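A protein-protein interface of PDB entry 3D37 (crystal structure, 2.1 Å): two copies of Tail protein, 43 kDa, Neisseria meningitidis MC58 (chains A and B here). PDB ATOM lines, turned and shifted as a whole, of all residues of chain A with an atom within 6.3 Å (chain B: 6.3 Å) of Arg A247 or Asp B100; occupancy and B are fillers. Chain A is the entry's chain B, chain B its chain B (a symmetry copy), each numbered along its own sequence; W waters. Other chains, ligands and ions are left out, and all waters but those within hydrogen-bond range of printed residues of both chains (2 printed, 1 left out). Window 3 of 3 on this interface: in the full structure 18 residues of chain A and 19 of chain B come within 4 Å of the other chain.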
ATOM      1  N   THR A 209       2.969 -16.963   3.175  1.00  0.00           N
ATOM      2  CA  THR A 209       3.331 -16.649   1.799  1.00  0.00           C
ATOM      3  C   THR A 209       3.120 -17.781   0.807  1.00  0.00           C
ATOM      4  O   THR A 209       3.453 -17.606  -0.342  1.00  0.00           O
ATOM      5  CB  THR A 209       4.809 -16.227   1.686  1.00  0.00           C
ATOM      6  OG1 THR A 209       5.651 -17.366   1.952  1.00  0.00           O
ATOM      7  CG2 THR A 209       5.117 -15.119   2.624  1.00  0.00           C
ATOM      8  N   ASP A 210       2.577 -18.934   1.208  1.00  0.00           N
ATOM      9  CA  ASP A 210       2.616 -20.102   0.303  1.00  0.00           C
ATOM     10  C   ASP A 210       1.838 -19.934  -1.031  1.00  0.00           C
ATOM     11  O   ASP A 210       2.120 -20.654  -1.993  1.00  0.00           O
ATOM     12  CB  ASP A 210       2.244 -21.444   0.972  1.00  0.00           C
ATOM     13  CG  ASP A 210       2.899 -22.705   0.223  1.00  0.00           C
ATOM     14  OD1 ASP A 210       4.169 -22.753  -0.046  1.00  0.00           O
ATOM     15  OD2 ASP A 210       2.133 -23.661  -0.117  1.00  0.00           O
ATOM     16  N   ASN A 211       0.889 -18.992  -1.084  1.00  0.00           N
ATOM     17  CA  ASN A 211       0.151 -18.743  -2.306  1.00  0.00           C
ATOM     18  C   ASN A 211       0.379 -17.327  -2.823  1.00  0.00           C
ATOM     19  O   ASN A 211      -0.466 -16.779  -3.516  1.00  0.00           O
ATOM     20  CB  ASN A 211      -1.348 -19.098  -2.139  1.00  0.00           C
ATOM     21  CG  ASN A 211      -1.617 -20.615  -2.259  1.00  0.00           C
ATOM     22  OD1 ASN A 211      -0.855 -21.337  -2.896  1.00  0.00           O
ATOM     23  ND2 ASN A 211      -2.723 -21.079  -1.696  1.00  0.00           N
ATOM     24  N   ARG A 212       1.523 -16.735  -2.507  1.00  0.00           N
ATOM     25  CA  ARG A 212       1.881 -15.534  -3.235  1.00  0.00           C
ATOM     26  C   ARG A 212       2.865 -15.881  -4.323  1.00  0.00           C
ATOM     27  O   ARG A 212       3.891 -16.493  -4.080  1.00  0.00           O
ATOM     28  CB  ARG A 212       2.384 -14.370  -2.419  1.00  0.00           C
ATOM     29  CG  ARG A 212       2.821 -14.643  -1.074  1.00  0.00           C
ATOM     30  CD  ARG A 212       2.957 -13.316  -0.315  1.00  0.00           C
ATOM     31  NE  ARG A 212       4.136 -12.532  -0.707  1.00  0.00           N
ATOM     32  CZ  ARG A 212       4.991 -11.987   0.169  1.00  0.00           C
ATOM     33  NH1 ARG A 212       4.789 -12.133   1.494  1.00  0.00           N
ATOM     34  NH2 ARG A 212       6.044 -11.284  -0.271  1.00  0.00           N
ATOM     35  N   PHE A 213       2.506 -15.473  -5.533  1.00  0.00           N
ATOM     36  CA  PHE A 213       3.216 -15.840  -6.721  1.00  0.00           C
ATOM     37  C   PHE A 213       3.715 -14.579  -7.362  1.00  0.00           C
ATOM     38  O   PHE A 213       3.173 -13.490  -7.143  1.00  0.00           O
ATOM     39  CB  PHE A 213       2.288 -16.621  -7.623  1.00  0.00           C
ATOM     40  CG  PHE A 213       1.711 -17.834  -6.961  1.00  0.00           C
ATOM     41  CD1 PHE A 213       2.548 -18.876  -6.571  1.00  0.00           C
ATOM     42  CD2 PHE A 213       0.337 -17.928  -6.702  1.00  0.00           C
ATOM     43  CE1 PHE A 213       2.031 -20.011  -5.986  1.00  0.00           C
ATOM     44  CE2 PHE A 213      -0.194 -19.053  -6.092  1.00  0.00           C
ATOM     45  CZ  PHE A 213       0.656 -20.105  -5.738  1.00  0.00           C
ATOM     46  N   SER A 214       4.809 -14.731  -8.092  1.00  0.00           N
ATOM     47  CA  SER A 214       5.491 -13.622  -8.738  1.00  0.00           C
ATOM     48  C   SER A 214       4.844 -13.372 -10.100  1.00  0.00           C
ATOM     49  O   SER A 214       4.742 -12.240 -10.537  1.00  0.00           O
ATOM     50  CB  SER A 214       6.982 -13.968  -8.895  1.00  0.00           C
ATOM     51  OG  SER A 214       7.134 -15.129  -9.715  1.00  0.00           O
ATOM     52  N   GLU A 215       4.439 -14.450 -10.762  1.00  0.00           N
ATOM     53  CA  GLU A 215       3.714 -14.400 -12.000  1.00  0.00           C
ATOM     54  C   GLU A 215       2.781 -15.595 -12.111  1.00  0.00           C
ATOM     55  O   GLU A 215       3.193 -16.732 -11.884  1.00  0.00           O
ATOM     56  CB  GLU A 215       4.661 -14.503 -13.192  1.00  0.00           C
ATOM     57  CG  GLU A 215       5.609 -13.324 -13.414  1.00  0.00           C
ATOM     58  CD  GLU A 215       6.138 -13.308 -14.857  1.00  0.00           C
ATOM     59  OE1 GLU A 215       5.582 -14.073 -15.695  1.00  0.00           O
ATOM     60  OE2 GLU A 215       7.087 -12.530 -15.140  1.00  0.00           O
ATOM     61  N   VAL A 216       1.546 -15.340 -12.529  1.00  0.00           N
ATOM     62  CA  VAL A 216       0.548 -16.383 -12.686  1.00  0.00           C
ATOM     63  C   VAL A 216      -0.055 -16.293 -14.108  1.00  0.00           C
ATOM     64  O   VAL A 216      -0.613 -15.254 -14.496  1.00  0.00           O
ATOM     65  CB  VAL A 216      -0.565 -16.308 -11.603  1.00  0.00           C
ATOM     66  CG1 VAL A 216      -1.485 -17.525 -11.695  1.00  0.00           C
ATOM     67  CG2 VAL A 216       0.041 -16.193 -10.219  1.00  0.00           C
ATOM     68  N   MET A 243       6.977  -8.577  -5.624  1.00  0.00           N
ATOM     69  CA  MET A 243       7.591  -9.923  -5.580  1.00  0.00           C
ATOM     70  C   MET A 243       8.950  -9.866  -6.259  1.00  0.00           C
ATOM     71  O   MET A 243       9.010  -9.663  -7.475  1.00  0.00           O
ATOM     72  CB  MET A 243       6.727 -10.974  -6.322  1.00  0.00           C
ATOM     73  CG  MET A 243       5.607 -11.611  -5.468  1.00  0.00           C
ATOM     74  SD  MET A 243       6.189 -12.801  -4.220  1.00  0.00           S
ATOM     75  CE  MET A 243       6.394 -14.286  -5.201  1.00  0.00           C
ATOM     76  N   LEU A 245      11.131 -12.567  -5.621  1.00  0.00           N
ATOM     77  CA  LEU A 245      11.471 -13.987  -5.750  1.00  0.00           C
ATOM     78  C   LEU A 245      10.705 -14.626  -6.900  1.00  0.00           C
ATOM     79  O   LEU A 245       9.570 -14.222  -7.206  1.00  0.00           O
ATOM     80  CB  LEU A 245      11.114 -14.741  -4.461  1.00  0.00           C
ATOM     81  CG  LEU A 245      11.531 -14.171  -3.085  1.00  0.00           C
ATOM     82  CD1 LEU A 245      10.710 -14.883  -1.991  1.00  0.00           C
ATOM     83  CD2 LEU A 245      13.052 -14.280  -2.867  1.00  0.00           C
ATOM     84  N   HIS A 246      11.306 -15.655  -7.496  1.00  0.00           N
ATOM     85  CA  HIS A 246      10.705 -16.359  -8.629  1.00  0.00           C
ATOM     86  C   HIS A 246       9.734 -17.436  -8.128  1.00  0.00           C
ATOM     87  O   HIS A 246      10.148 -18.423  -7.523  1.00  0.00           O
ATOM     88  CB  HIS A 246      11.804 -16.973  -9.505  1.00  0.00           C
ATOM     89  CG  HIS A 246      11.295 -17.710 -10.708  1.00  0.00           C
ATOM     90  ND1 HIS A 246      10.595 -17.094 -11.723  1.00  0.00           N
ATOM     91  CD2 HIS A 246      11.414 -19.010 -11.071  1.00  0.00           C
ATOM     92  CE1 HIS A 246      10.299 -17.984 -12.657  1.00  0.00           C
ATOM     93  NE2 HIS A 246      10.779 -19.156 -12.282  1.00  0.00           N
ATOM     94  N   ARG A 247       8.437 -17.227  -8.358  1.00  0.00           N
ATOM     95  CA  ARG A 247       7.440 -18.234  -8.007  1.00  0.00           C
ATOM     96  C   ARG A 247       6.329 -18.251  -9.024  1.00  0.00           C
ATOM     97  O   ARG A 247       5.217 -17.823  -8.720  1.00  0.00           O
ATOM     98  CB  ARG A 247       6.855 -17.980  -6.602  1.00  0.00           C
ATOM     99  CG  ARG A 247       7.740 -18.358  -5.462  1.00  0.00           C
ATOM    100  CD  ARG A 247       6.937 -18.403  -4.164  1.00  0.00           C
ATOM    101  NE  ARG A 247       6.502 -19.742  -3.727  1.00  0.00           N
ATOM    102  CZ  ARG A 247       5.264 -20.053  -3.319  1.00  0.00           C
ATOM    103  NH1 ARG A 247       4.290 -19.144  -3.349  1.00  0.00           N
ATOM    104  NH2 ARG A 247       4.996 -21.290  -2.899  1.00  0.00           N
ATOM    105  N   PRO A 248       6.615 -18.757 -10.241  1.00  0.00           N
ATOM    106  CA  PRO A 248       5.635 -18.735 -11.320  1.00  0.00           C
ATOM    107  C   PRO A 248       4.566 -19.780 -11.081  1.00  0.00           C
ATOM    108  O   PRO A 248       4.820 -20.796 -10.424  1.00  0.00           O
ATOM    109  CB  PRO A 248       6.451 -19.141 -12.547  1.00  0.00           C
ATOM    110  CG  PRO A 248       7.480 -20.072 -11.984  1.00  0.00           C
ATOM    111  CD  PRO A 248       7.857 -19.443 -10.657  1.00  0.00           C
ATOM    112  N   LYS A 249       3.376 -19.539 -11.599  1.00  0.00           N
ATOM    113  CA  LYS A 249       2.323 -20.536 -11.536  1.00  0.00           C
ATOM    114  C   LYS A 249       1.512 -20.468 -12.811  1.00  0.00           C
ATOM    115  O   LYS A 249       1.420 -19.427 -13.434  1.00  0.00           O
ATOM    116  CB  LYS A 249       1.412 -20.338 -10.320  1.00  0.00           C
ATOM    117  CG  LYS A 249       0.456 -21.538 -10.085  1.00  0.00           C
ATOM    118  CD  LYS A 249      -0.321 -21.446  -8.786  1.00  0.00           C
ATOM    119  CE  LYS A 249      -1.411 -22.503  -8.715  1.00  0.00           C
ATOM    120  NZ  LYS A 249      -0.910 -23.770  -8.088  1.00  0.00           N
ATOM    121  N   ARG B  92      11.663 -22.774   5.265  1.00  0.00           N
ATOM    122  CA  ARG B  92      12.417 -23.823   4.669  1.00  0.00           C
ATOM    123  C   ARG B  92      13.640 -23.246   3.975  1.00  0.00           C
ATOM    124  O   ARG B  92      13.725 -22.076   3.765  1.00  0.00           O
ATOM    125  CB  ARG B  92      11.544 -24.519   3.649  1.00  0.00           C
ATOM    126  CG  ARG B  92      10.346 -25.188   4.249  1.00  0.00           C
ATOM    127  CD  ARG B  92       9.474 -25.771   3.169  1.00  0.00           C
ATOM    128  NE  ARG B  92       8.846 -24.705   2.416  1.00  0.00           N
ATOM    129  CZ  ARG B  92       8.323 -24.835   1.210  1.00  0.00           C
ATOM    130  NH1 ARG B  92       8.300 -26.016   0.588  1.00  0.00           N
ATOM    131  NH2 ARG B  92       7.841 -23.761   0.626  1.00  0.00           N
ATOM    132  N   ALA B  95      15.512 -25.287  -1.263  1.00  0.00           N
ATOM    133  CA  ALA B  95      14.769 -26.398  -1.921  1.00  0.00           C
ATOM    134  C   ALA B  95      13.282 -26.152  -1.916  1.00  0.00           C
ATOM    135  O   ALA B  95      12.568 -26.764  -2.702  1.00  0.00           O
ATOM    136  CB  ALA B  95      15.085 -27.767  -1.258  1.00  0.00           C
ATOM    137  N   GLY B  96      12.782 -25.262  -1.039  1.00  0.00           N
ATOM    138  CA  GLY B  96      11.340 -24.945  -0.961  1.00  0.00           C
ATOM    139  C   GLY B  96      10.775 -24.508  -2.302  1.00  0.00           C
ATOM    140  O   GLY B  96       9.700 -24.909  -2.717  1.00  0.00           O
ATOM    141  N   PHE B  97      11.566 -23.745  -3.028  1.00  0.00           N
ATOM    142  CA  PHE B  97      11.235 -23.338  -4.377  1.00  0.00           C
ATOM    143  C   PHE B  97      11.072 -24.500  -5.333  1.00  0.00           C
ATOM    144  O   PHE B  97      10.175 -24.496  -6.146  1.00  0.00           O
ATOM    145  CB  PHE B  97      12.330 -22.436  -4.953  1.00  0.00           C
ATOM    146  CG  PHE B  97      12.383 -21.047  -4.343  1.00  0.00           C
ATOM    147  CD1 PHE B  97      11.336 -20.136  -4.552  1.00  0.00           C
ATOM    148  CD2 PHE B  97      13.502 -20.632  -3.653  1.00  0.00           C
ATOM    149  CE1 PHE B  97      11.381 -18.853  -4.021  1.00  0.00           C
ATOM    150  CE2 PHE B  97      13.557 -19.368  -3.117  1.00  0.00           C
ATOM    151  CZ  PHE B  97      12.486 -18.456  -3.296  1.00  0.00           C
ATOM    152  N   LEU B  98      11.992 -25.461  -5.256  1.00  0.00           N
ATOM    153  CA  LEU B  98      12.057 -26.524  -6.237  1.00  0.00           C
ATOM    154  C   LEU B  98      11.031 -27.603  -5.853  1.00  0.00           C
ATOM    155  O   LEU B  98      10.490 -28.260  -6.703  1.00  0.00           O
ATOM    156  CB  LEU B  98      13.456 -27.128  -6.267  1.00  0.00           C
ATOM    157  CG  LEU B  98      14.719 -26.313  -6.568  1.00  0.00           C
ATOM    158  CD1 LEU B  98      15.496 -27.090  -7.571  1.00  0.00           C
ATOM    159  CD2 LEU B  98      14.520 -24.896  -7.048  1.00  0.00           C
ATOM    160  N   VAL B  99      10.755 -27.716  -4.556  1.00  0.00           N
ATOM    161  CA  VAL B  99       9.687 -28.538  -4.004  1.00  0.00           C
ATOM    162  C   VAL B  99       8.329 -28.012  -4.472  1.00  0.00           C
ATOM    163  O   VAL B  99       7.511 -28.779  -4.841  1.00  0.00           O
ATOM    164  CB  VAL B  99       9.784 -28.669  -2.426  1.00  0.00           C
ATOM    165  CG1 VAL B  99       8.460 -29.179  -1.728  1.00  0.00           C
ATOM    166  CG2 VAL B  99      11.007 -29.575  -1.996  1.00  0.00           C
ATOM    167  N   ASP B 100       8.116 -26.704  -4.479  1.00  0.00           N
ATOM    168  CA  ASP B 100       6.790 -26.162  -4.795  1.00  0.00           C
ATOM    169  C   ASP B 100       6.524 -26.078  -6.291  1.00  0.00           C
ATOM    170  O   ASP B 100       5.392 -26.210  -6.699  1.00  0.00           O
ATOM    171  CB  ASP B 100       6.568 -24.761  -4.181  1.00  0.00           C
ATOM    172  CG  ASP B 100       6.635 -24.748  -2.652  1.00  0.00           C
ATOM    173  OD1 ASP B 100       6.577 -25.792  -1.991  1.00  0.00           O
ATOM    174  OD2 ASP B 100       6.809 -23.644  -2.092  1.00  0.00           O
ATOM    175  N   CYS B 101       7.556 -25.844  -7.101  1.00  0.00           N
ATOM    176  CA  CYS B 101       7.336 -25.403  -8.474  1.00  0.00           C
ATOM    177  C   CYS B 101       7.424 -26.588  -9.437  1.00  0.00           C
ATOM    178  O   CYS B 101       8.032 -27.596  -9.132  1.00  0.00           O
ATOM    179  CB  CYS B 101       8.305 -24.263  -8.822  1.00  0.00           C
ATOM    180  SG  CYS B 101       8.267 -22.821  -7.588  1.00  0.00           S
ATOM    181  N   SER B 102       6.737 -26.461 -10.575  1.00  0.00           N
ATOM    182  CA  SER B 102       6.682 -27.477 -11.654  1.00  0.00           C
ATOM    183  C   SER B 102       7.983 -27.594 -12.395  1.00  0.00           C
ATOM    184  O   SER B 102       8.638 -26.596 -12.704  1.00  0.00           O
ATOM    185  CB  SER B 102       5.584 -27.131 -12.651  1.00  0.00           C
ATOM    186  OG  SER B 102       4.333 -27.322 -11.986  1.00  0.00           O
ATOM    187  N   TRP B 124      16.144 -20.063 -10.215  1.00  0.00           N
ATOM    188  CA  TRP B 124      16.282 -19.522  -8.892  1.00  0.00           C
ATOM    189  C   TRP B 124      17.723 -19.093  -8.607  1.00  0.00           C
ATOM    190  O   TRP B 124      18.504 -19.859  -8.049  1.00  0.00           O
ATOM    191  CB  TRP B 124      15.756 -20.550  -7.863  1.00  0.00           C
ATOM    192  CG  TRP B 124      14.266 -20.823  -8.104  1.00  0.00           C
ATOM    193  CD1 TRP B 124      13.213 -20.079  -7.636  1.00  0.00           C
ATOM    194  CD2 TRP B 124      13.689 -21.858  -8.910  1.00  0.00           C
ATOM    195  NE1 TRP B 124      12.023 -20.593  -8.085  1.00  0.00           N
ATOM    196  CE2 TRP B 124      12.280 -21.690  -8.861  1.00  0.00           C
ATOM    197  CE3 TRP B 124      14.211 -22.931  -9.645  1.00  0.00           C
ATOM    198  CZ2 TRP B 124      11.410 -22.536  -9.520  1.00  0.00           C
ATOM    199  CZ3 TRP B 124      13.338 -23.776 -10.296  1.00  0.00           C
ATOM    200  CH2 TRP B 124      11.954 -23.568 -10.250  1.00  0.00           C
ATOM    201  N   THR B 150       7.280 -31.998  -9.646  1.00  0.00           N
ATOM    202  CA  THR B 150       7.961 -30.791  -9.179  1.00  0.00           C
ATOM    203  C   THR B 150       9.395 -30.823  -9.665  1.00  0.00           C
ATOM    204  O   THR B 150       9.899 -31.859 -10.094  1.00  0.00           O
ATOM    205  CB  THR B 150       7.952 -30.679  -7.662  1.00  0.00           C
ATOM    206  OG1 THR B 150       8.649 -31.789  -7.092  1.00  0.00           O
ATOM    207  CG2 THR B 150       6.525 -30.634  -7.112  1.00  0.00           C
ATOM    208  N   VAL B 151      10.059 -29.688  -9.539  1.00  0.00           N
ATOM    209  CA  VAL B 151      11.461 -29.592  -9.812  1.00  0.00           C
ATOM    210  C   VAL B 151      12.283 -30.521  -8.898  1.00  0.00           C
ATOM    211  O   VAL B 151      13.226 -31.140  -9.400  1.00  0.00           O
ATOM    212  CB  VAL B 151      11.991 -28.139  -9.743  1.00  0.00           C
ATOM    213  CG1 VAL B 151      13.493 -28.134 -10.079  1.00  0.00           C
ATOM    214  CG2 VAL B 151      11.191 -27.243 -10.731  1.00  0.00           C
ATOM    215  N   TRP B 152      11.876 -30.685  -7.624  1.00  0.00           N
ATOM    216  CA  TRP B 152      12.628 -31.496  -6.696  1.00  0.00           C
ATOM    217  C   TRP B 152      12.475 -32.969  -7.066  1.00  0.00           C
ATOM    218  O   TRP B 152      13.429 -33.749  -7.000  1.00  0.00           O
ATOM    219  CB  TRP B 152      12.216 -31.253  -5.223  1.00  0.00           C
ATOM    220  CG  TRP B 152      13.248 -31.845  -4.282  1.00  0.00           C
ATOM    221  CD1 TRP B 152      13.199 -33.066  -3.649  1.00  0.00           C
ATOM    222  CD2 TRP B 152      14.548 -31.291  -3.982  1.00  0.00           C
ATOM    223  NE1 TRP B 152      14.370 -33.282  -2.950  1.00  0.00           N
ATOM    224  CE2 TRP B 152      15.202 -32.204  -3.109  1.00  0.00           C
ATOM    225  CE3 TRP B 152      15.199 -30.094  -4.337  1.00  0.00           C
ATOM    226  CZ2 TRP B 152      16.464 -31.960  -2.574  1.00  0.00           C
ATOM    227  CZ3 TRP B 152      16.456 -29.836  -3.813  1.00  0.00           C
ATOM    228  CH2 TRP B 152      17.084 -30.780  -2.926  1.00  0.00           C
HETATM  229  O   HOH W   1       8.674 -21.708  -3.013  1.00  0.00           O
HETATM  230  O   HOH W   2       6.084 -23.357 -10.978  1.00  0.00           O
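The backbone carbonyl oxygen of Thr A209 is in hydrogen-bond range of the guanidinium group of Arg A247, 3.5 Å away.
OD1 of Asp A210 is in salt-bridge range of NH2 of Arg A247 (3.3 Å).
The guanidinium group of Arg A247 lies within hydrogen-bond range of the backbone carbonyl oxygen of Arg A212 (2.8 Å).
OG of Ser A214 sits at hydrogen-bond distance from N of Arg A247, at 2.8 Å.
NH2 of Arg B92 is in salt-bridge range of OD2 of Asp B100.
The backbone carbonyl oxygen of Phe B97 is in hydrogen-bond range of the side-chain sulfur of Cys B101.
No position is printed for both chains.
Of the 6 pairs that touch across the chains among the printed residues, none has its exchanged pair printed and touching as well.
The guanidinium group (NH2) of Arg B92 is in salt-bridge range of the side-chain carboxylate (OD1) of Asp A210, at 3.9 Å.
The indole nitrogen (NE1) of Trp B124 sits at hydrogen-bond distance from the backbone carbonyl oxygen (O) of His A246 (2.9 Å).
The side-chain carboxylate of Asp B100 lies within salt-bridge range of the guanidinium group of Arg A247, 3.1 Å away.
OD1 of Asp A210 sits close to OD2 of Asp B100 (3.5 Å).
Water W1 lies within hydrogen-bond range of the side-chain carboxylate (OD2) of Asp B100 (2.8 Å), the guanidinium group (NE) of Arg A247 (3.0 Å) and the backbone carbonyl oxygen (O) of Gly B96 (3.4 Å).
Water W2 lies within hydrogen-bond range of O of Pro A248 (2.9 Å) and N of Ser B102 (3.2 Å).
Asp B100 touches just these residues of chain A: Asp A210 and Arg A247.
Printed residues of chain A within 4 Å of Trp B124: His A246 (2.9 Å).
Of the printed residues of chain A, Phe B97 touches His A246 and Arg A247.
Of the printed residues of chain A, Arg B92 touches Asp A210 (3.9 Å).
Printed residues of chain B within 4 Å of His A246: Phe B97 and Trp B124.
Val B99 touches none of the printed residues of chain A.
Ala B95 touches none of the printed residues of chain A.
The nearest printed residue of chain A that does not touch Trp B124 is Pro A248 (4.8 Å).
Hydrophobic or aromatic side chains of chain B that line the printed part of chain A: Phe B97 and Trp B124.
Printed residues of chain A that touch a printed residue of chain B: Asp A210, His A246 and Arg A247.
Hydrophobic or aromatic side chains of chain A that line the printed part of chain B: His A246.
Among the printed residues, 6 pairs touch across the chains.
Phe B97 touches His A246 (CD1 to O, 3.6 Å).
CE1 of Phe B97 touches CG of Arg A247, 3.9 Å away.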
